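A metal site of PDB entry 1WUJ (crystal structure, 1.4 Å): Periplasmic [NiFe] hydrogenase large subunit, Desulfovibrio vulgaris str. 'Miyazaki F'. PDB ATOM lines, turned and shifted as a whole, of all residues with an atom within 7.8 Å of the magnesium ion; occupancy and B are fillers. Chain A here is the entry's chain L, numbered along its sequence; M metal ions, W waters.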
ATOM      1  N   GLU A  44     -19.658 -30.514   4.808  1.00  0.00           N
ATOM      2  CA  GLU A  44     -20.023 -31.004   6.132  1.00  0.00           C
ATOM      3  C   GLU A  44     -21.265 -31.902   6.072  1.00  0.00           C
ATOM      4  O   GLU A  44     -21.392 -32.893   6.800  1.00  0.00           O
ATOM      5  CB  GLU A  44     -20.242 -29.862   7.139  1.00  0.00           C
ATOM      6  CG  GLU A  44     -18.953 -29.093   7.408  1.00  0.00           C
ATOM      7  CD  GLU A  44     -19.218 -27.635   7.798  1.00  0.00           C
ATOM      8  OE1 GLU A  44     -20.281 -27.092   7.439  1.00  0.00           O
ATOM      9  OE2 GLU A  44     -18.306 -27.034   8.438  1.00  0.00           O
ATOM     10  N   GLU A 319     -19.938 -20.243  15.915  1.00  0.00           N
ATOM     11  CA  GLU A 319     -20.164 -19.787  14.535  1.00  0.00           C
ATOM     12  C   GLU A 319     -21.620 -19.319  14.377  1.00  0.00           C
ATOM     13  O   GLU A 319     -22.551 -20.085  14.585  1.00  0.00           O
ATOM     14  CB  GLU A 319     -19.861 -20.865  13.514  1.00  0.00           C
ATOM     15  CG  GLU A 319     -18.419 -21.273  13.478  1.00  0.00           C
ATOM     16  CD  GLU A 319     -18.163 -22.248  12.329  1.00  0.00           C
ATOM     17  OE1 GLU A 319     -17.600 -21.858  11.286  1.00  0.00           O
ATOM     18  OE2 GLU A 319     -18.563 -23.414  12.483  1.00  0.00           O
ATOM     19  N   TYR A 326     -28.227 -19.574   6.232  1.00  0.00           N
ATOM     20  CA  TYR A 326     -28.490 -20.794   6.943  1.00  0.00           C
ATOM     21  C   TYR A 326     -29.732 -20.552   7.781  1.00  0.00           C
ATOM     22  O   TYR A 326     -30.112 -19.424   8.010  1.00  0.00           O
ATOM     23  CB  TYR A 326     -27.343 -21.265   7.865  1.00  0.00           C
ATOM     24  CG  TYR A 326     -26.111 -21.542   7.017  1.00  0.00           C
ATOM     25  CD1 TYR A 326     -25.100 -20.565   6.892  1.00  0.00           C
ATOM     26  CD2 TYR A 326     -25.967 -22.750   6.324  1.00  0.00           C
ATOM     27  CE1 TYR A 326     -23.984 -20.802   6.130  1.00  0.00           C
ATOM     28  CE2 TYR A 326     -24.837 -22.970   5.546  1.00  0.00           C
ATOM     29  CZ  TYR A 326     -23.853 -22.005   5.457  1.00  0.00           C
ATOM     30  OH  TYR A 326     -22.739 -22.240   4.659  1.00  0.00           O
ATOM     31  N   PRO A 334     -18.561 -25.617  17.321  1.00  0.00           N
ATOM     32  CA  PRO A 334     -18.508 -26.616  16.222  1.00  0.00           C
ATOM     33  C   PRO A 334     -18.742 -28.072  16.600  1.00  0.00           C
ATOM     34  O   PRO A 334     -19.151 -28.897  15.777  1.00  0.00           O
ATOM     35  CB  PRO A 334     -17.112 -26.479  15.646  1.00  0.00           C
ATOM     36  CG  PRO A 334     -16.427 -25.441  16.413  1.00  0.00           C
ATOM     37  CD  PRO A 334     -17.350 -24.815  17.407  1.00  0.00           C
ATOM     38  N   GLN A 338     -24.151 -26.887  13.079  1.00  0.00           N
ATOM     39  CA  GLN A 338     -25.244 -27.117  12.175  1.00  0.00           C
ATOM     40  C   GLN A 338     -24.941 -26.474  10.817  1.00  0.00           C
ATOM     41  O   GLN A 338     -24.444 -25.337  10.819  1.00  0.00           O
ATOM     42  CB  GLN A 338     -26.575 -26.536  12.676  1.00  0.00           C
ATOM     43  CG  GLN A 338     -27.013 -27.153  14.014  1.00  0.00           C
ATOM     44  CD  GLN A 338     -28.325 -26.533  14.525  1.00  0.00           C
ATOM     45  OE1 GLN A 338     -29.284 -27.279  14.729  1.00  0.00           O
ATOM     46  NE2 GLN A 338     -28.274 -25.217  14.688  1.00  0.00           N
ATOM     47  N   THR A 339     -25.259 -27.209   9.756  1.00  0.00           N
ATOM     48  CA  THR A 339     -25.069 -26.668   8.415  1.00  0.00           C
ATOM     49  C   THR A 339     -26.354 -26.916   7.638  1.00  0.00           C
ATOM     50  O   THR A 339     -26.485 -27.960   7.012  1.00  0.00           O
ATOM     51  CB  THR A 339     -23.828 -27.278   7.752  1.00  0.00           C
ATOM     52  OG1 THR A 339     -22.752 -27.090   8.668  1.00  0.00           O
ATOM     53  CG2 THR A 339     -23.542 -26.582   6.437  1.00  0.00           C
ATOM     54  N   TRP A 354     -22.603 -17.083   2.210  1.00  0.00           N
ATOM     55  CA  TRP A 354     -22.588 -18.502   2.524  1.00  0.00           C
ATOM     56  C   TRP A 354     -21.569 -18.827   3.624  1.00  0.00           C
ATOM     57  O   TRP A 354     -21.559 -19.962   4.110  1.00  0.00           O
ATOM     58  CB  TRP A 354     -22.298 -19.393   1.301  1.00  0.00           C
ATOM     59  CG  TRP A 354     -23.435 -19.466   0.334  1.00  0.00           C
ATOM     60  CD1 TRP A 354     -23.533 -18.942  -0.917  1.00  0.00           C
ATOM     61  CD2 TRP A 354     -24.693 -20.137   0.559  1.00  0.00           C
ATOM     62  NE1 TRP A 354     -24.745 -19.237  -1.494  1.00  0.00           N
ATOM     63  CE2 TRP A 354     -25.473 -19.965  -0.603  1.00  0.00           C
ATOM     64  CE3 TRP A 354     -25.198 -20.857   1.624  1.00  0.00           C
ATOM     65  CZ2 TRP A 354     -26.757 -20.487  -0.718  1.00  0.00           C
ATOM     66  CZ3 TRP A 354     -26.480 -21.384   1.516  1.00  0.00           C
ATOM     67  CH2 TRP A 354     -27.234 -21.196   0.360  1.00  0.00           C
ATOM     68  N   LYS A 356     -20.381 -18.802   7.457  1.00  0.00           N
ATOM     69  CA  LYS A 356     -20.762 -18.543   8.850  1.00  0.00           C
ATOM     70  C   LYS A 356     -19.850 -17.445   9.385  1.00  0.00           C
ATOM     71  O   LYS A 356     -18.843 -17.096   8.725  1.00  0.00           O
ATOM     72  CB  LYS A 356     -20.649 -19.805   9.709  1.00  0.00           C
ATOM     73  CG  LYS A 356     -21.509 -20.964   9.205  1.00  0.00           C
ATOM     74  CD  LYS A 356     -21.331 -22.235  10.002  1.00  0.00           C
ATOM     75  CE  LYS A 356     -22.211 -23.394   9.554  1.00  0.00           C
ATOM     76  NZ  LYS A 356     -21.792 -24.672  10.193  1.00  0.00           N
ATOM     77  N   PRO A 358     -17.594 -16.816  12.513  1.00  0.00           N
ATOM     78  CA  PRO A 358     -17.009 -17.282  13.765  1.00  0.00           C
ATOM     79  C   PRO A 358     -16.686 -16.099  14.670  1.00  0.00           C
ATOM     80  O   PRO A 358     -16.164 -15.103  14.170  1.00  0.00           O
ATOM     81  CB  PRO A 358     -15.750 -17.993  13.315  1.00  0.00           C
ATOM     82  CG  PRO A 358     -15.919 -18.252  11.840  1.00  0.00           C
ATOM     83  CD  PRO A 358     -16.696 -17.026  11.372  1.00  0.00           C
ATOM     84  N   SER A 465      -9.485 -25.381  12.087  1.00  0.00           N
ATOM     85  CA  SER A 465      -9.872 -26.433  13.017  1.00  0.00           C
ATOM     86  C   SER A 465     -10.938 -27.300  12.350  1.00  0.00           C
ATOM     87  O   SER A 465     -11.839 -26.792  11.707  1.00  0.00           O
ATOM     88  CB  SER A 465     -10.290 -25.874  14.386  1.00  0.00           C
ATOM     89  OG  SER A 465     -11.301 -24.898  14.330  1.00  0.00           O
ATOM     90  N   TRP A 467     -13.515 -30.537  13.458  1.00  0.00           N
ATOM     91  CA  TRP A 467     -14.171 -31.050  14.651  1.00  0.00           C
ATOM     92  C   TRP A 467     -15.070 -32.235  14.341  1.00  0.00           C
ATOM     93  O   TRP A 467     -15.941 -32.083  13.493  1.00  0.00           O
ATOM     94  CB  TRP A 467     -15.000 -29.939  15.265  1.00  0.00           C
ATOM     95  CG  TRP A 467     -14.312 -28.632  15.506  1.00  0.00           C
ATOM     96  CD1 TRP A 467     -13.931 -27.717  14.578  1.00  0.00           C
ATOM     97  CD2 TRP A 467     -13.923 -28.128  16.797  1.00  0.00           C
ATOM     98  NE1 TRP A 467     -13.341 -26.658  15.233  1.00  0.00           N
ATOM     99  CE2 TRP A 467     -13.318 -26.886  16.581  1.00  0.00           C
ATOM    100  CE3 TRP A 467     -14.021 -28.598  18.101  1.00  0.00           C
ATOM    101  CZ2 TRP A 467     -12.825 -26.109  17.626  1.00  0.00           C
ATOM    102  CZ3 TRP A 467     -13.542 -27.842  19.135  1.00  0.00           C
ATOM    103  CH2 TRP A 467     -12.955 -26.612  18.877  1.00  0.00           C
ATOM    104  N   PHE A 478     -19.364 -33.467  11.479  1.00  0.00           N
ATOM    105  CA  PHE A 478     -18.023 -33.026  11.128  1.00  0.00           C
ATOM    106  C   PHE A 478     -18.132 -31.548  10.755  1.00  0.00           C
ATOM    107  O   PHE A 478     -18.903 -31.229   9.838  1.00  0.00           O
ATOM    108  CB  PHE A 478     -17.462 -33.840   9.965  1.00  0.00           C
ATOM    109  CG  PHE A 478     -15.942 -33.819   9.905  1.00  0.00           C
ATOM    110  CD1 PHE A 478     -15.297 -32.688   9.432  1.00  0.00           C
ATOM    111  CD2 PHE A 478     -15.203 -34.903  10.347  1.00  0.00           C
ATOM    112  CE1 PHE A 478     -13.882 -32.663   9.441  1.00  0.00           C
ATOM    113  CE2 PHE A 478     -13.809 -34.909  10.352  1.00  0.00           C
ATOM    114  CZ  PHE A 478     -13.156 -33.768   9.872  1.00  0.00           C
ATOM    115  N   GLN A 479     -17.409 -30.697  11.438  1.00  0.00           N
ATOM    116  CA  GLN A 479     -17.487 -29.274  11.194  1.00  0.00           C
ATOM    117  C   GLN A 479     -16.100 -28.708  10.934  1.00  0.00           C
ATOM    118  O   GLN A 479     -15.154 -28.999  11.673  1.00  0.00           O
ATOM    119  CB  GLN A 479     -18.142 -28.584  12.392  1.00  0.00           C
ATOM    120  CG  GLN A 479     -19.607 -28.954  12.575  1.00  0.00           C
ATOM    121  CD  GLN A 479     -20.511 -28.333  11.546  1.00  0.00           C
ATOM    122  OE1 GLN A 479     -20.280 -27.223  11.055  1.00  0.00           O
ATOM    123  NE2 GLN A 479     -21.562 -29.094  11.245  1.00  0.00           N
ATOM    124  N   LEU A 480     -16.051 -27.915   9.866  1.00  0.00           N
ATOM    125  CA  LEU A 480     -14.835 -27.187   9.555  1.00  0.00           C
ATOM    126  C   LEU A 480     -15.027 -25.726   9.952  1.00  0.00           C
ATOM    127  O   LEU A 480     -16.034 -25.133   9.602  1.00  0.00           O
ATOM    128  CB  LEU A 480     -14.419 -27.212   8.083  1.00  0.00           C
ATOM    129  CG  LEU A 480     -14.104 -28.550   7.452  1.00  0.00           C
ATOM    130  CD1 LEU A 480     -15.322 -29.427   7.376  1.00  0.00           C
ATOM    131  CD2 LEU A 480     -13.555 -28.333   6.045  1.00  0.00           C
ATOM    132  N   VAL A 481     -14.041 -25.128  10.608  1.00  0.00           N
ATOM    133  CA  VAL A 481     -14.025 -23.727  10.932  1.00  0.00           C
ATOM    134  C   VAL A 481     -12.671 -23.242  10.368  1.00  0.00           C
ATOM    135  O   VAL A 481     -11.636 -23.656  10.867  1.00  0.00           O
ATOM    136  CB  VAL A 481     -14.114 -23.388  12.420  1.00  0.00           C
ATOM    137  CG1 VAL A 481     -14.257 -21.898  12.622  1.00  0.00           C
ATOM    138  CG2 VAL A 481     -15.277 -24.127  13.026  1.00  0.00           C
ATOM    139  N   VAL A 482     -12.709 -22.440   9.305  1.00  0.00           N
ATOM    140  CA  VAL A 482     -11.526 -22.253   8.455  1.00  0.00           C
ATOM    141  C   VAL A 482     -11.041 -20.819   8.576  1.00  0.00           C
ATOM    142  O   VAL A 482     -11.800 -19.938   8.929  1.00  0.00           O
ATOM    143  CB  VAL A 482     -11.921 -22.687   7.027  1.00  0.00           C
ATOM    144  CG1 VAL A 482     -10.782 -22.757   6.052  1.00  0.00           C
ATOM    145  CG2 VAL A 482     -12.512 -24.107   7.109  1.00  0.00           C
ATOM    146  N   THR A 485     -12.996 -18.216   7.072  1.00  0.00           N
ATOM    147  CA  THR A 485     -14.298 -18.028   7.708  1.00  0.00           C
ATOM    148  C   THR A 485     -14.215 -16.934   8.777  1.00  0.00           C
ATOM    149  O   THR A 485     -15.039 -16.034   8.869  1.00  0.00           O
ATOM    150  CB  THR A 485     -14.802 -19.353   8.343  1.00  0.00           C
ATOM    151  OG1 THR A 485     -14.477 -20.452   7.504  1.00  0.00           O
ATOM    152  CG2 THR A 485     -16.313 -19.296   8.521  1.00  0.00           C
ATOM    153  N   CYS A 531     -12.405 -22.414   0.982  1.00  0.00           N
ATOM    154  CA  CYS A 531     -12.088 -22.634   2.384  1.00  0.00           C
ATOM    155  C   CYS A 531     -13.152 -22.066   3.297  1.00  0.00           C
ATOM    156  O   CYS A 531     -13.644 -22.708   4.239  1.00  0.00           O
ATOM    157  CB  CYS A 531     -10.755 -21.925   2.775  1.00  0.00           C
ATOM    158  SG  CYS A 531      -9.376 -23.108   2.544  1.00  0.00           S
ATOM    159  N   GLY A 532     -13.505 -20.797   3.103  1.00  0.00           N
ATOM    160  CA  GLY A 532     -14.312 -20.167   4.121  1.00  0.00           C
ATOM    161  C   GLY A 532     -15.695 -20.787   4.251  1.00  0.00           C
ATOM    162  O   GLY A 532     -16.270 -20.852   5.332  1.00  0.00           O
ATOM    163  N   VAL A 533     -16.221 -21.220   3.098  1.00  0.00           N
ATOM    164  CA  VAL A 533     -17.598 -21.744   3.032  1.00  0.00           C
ATOM    165  C   VAL A 533     -17.705 -23.256   3.070  1.00  0.00           C
ATOM    166  O   VAL A 533     -18.557 -23.849   3.763  1.00  0.00           O
ATOM    167  CB  VAL A 533     -18.340 -21.345   1.734  1.00  0.00           C
ATOM    168  CG1 VAL A 533     -19.754 -21.943   1.712  1.00  0.00           C
ATOM    169  CG2 VAL A 533     -18.395 -19.830   1.564  1.00  0.00           C
ATOM    170  N   HIS A 534     -16.806 -23.981   2.351  1.00  0.00           N
ATOM    171  CA  HIS A 534     -16.816 -25.448   2.257  1.00  0.00           C
ATOM    172  C   HIS A 534     -18.253 -25.992   2.014  1.00  0.00           C
ATOM    173  O   HIS A 534     -18.945 -25.307   1.102  1.00  0.00           O
ATOM    174  CB  HIS A 534     -16.097 -26.166   3.416  1.00  0.00           C
ATOM    175  CG  HIS A 534     -16.298 -25.596   4.773  1.00  0.00           C
ATOM    176  ND1 HIS A 534     -15.652 -24.435   5.145  1.00  0.00           N
ATOM    177  CD2 HIS A 534     -17.123 -25.897   5.786  1.00  0.00           C
ATOM    178  CE1 HIS A 534     -16.035 -24.087   6.363  1.00  0.00           C
ATOM    179  NE2 HIS A 534     -16.935 -24.967   6.771  1.00  0.00           N
ATOM    180  OXT HIS A 534     -18.699 -26.990   2.594  1.00  0.00           O
HETATM  181 MG    MG M   1     -17.925 -24.960   8.712  1.00  0.00          MG
HETATM  182  O   HOH W   1     -19.835 -24.568   7.885  1.00  0.00           O
HETATM  183  O   HOH W   2     -18.822 -25.112  10.589  1.00  0.00           O
HETATM  184  O   HOH W   3     -17.628 -22.859   8.902  1.00  0.00           O
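A ring nitrogen (ND1) of His 534 sits at hydrogen-bond distance from the backbone carbonyl oxygen (O) of Cys 531 (2.8 Å).
The side-chain carboxylate of Glu 44 is in hydrogen-bond range of the side-chain hydroxyl of Thr 339.
OE1 of Gln 479 lies close to OE2 of Glu 44.
The side-chain carboxylate of Glu 44 lies within salt-bridge range of the side-chain amino group of Lys 356 (3.97 Å).
Three residues have an atom within 4 Å of the magnesium ion: Glu 44, Leu 480 and His 534.
The nearest printed residue that does not touch the magnesium ion is Gln 479 (4.02 Å).
The magnesium ion is bound by water W2, 2.1 Å away.
The magnesium ion is bound by O of Leu 480.
Water W1 binds the magnesium ion (2.1 Å).
The magnesium ion is bound by the side-chain carboxylate (OE2) of Glu 44.
Water W3 is bound to the magnesium ion.
NE2 of His 534 binds the magnesium ion, at 2.2 Å.
Water W1 lies within hydrogen-bond range of the side-chain carboxylate (OE1) of Glu 44 (2.6 Å) and the side-chain amino group (NZ) of Lys 356 (3.0 Å).
Water W2 lies within hydrogen-bond range of OE2 of Glu 319 (2.6 Å), OE1 of Gln 479 (2.6 Å) and NZ of Lys 356 (3.0 Å).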
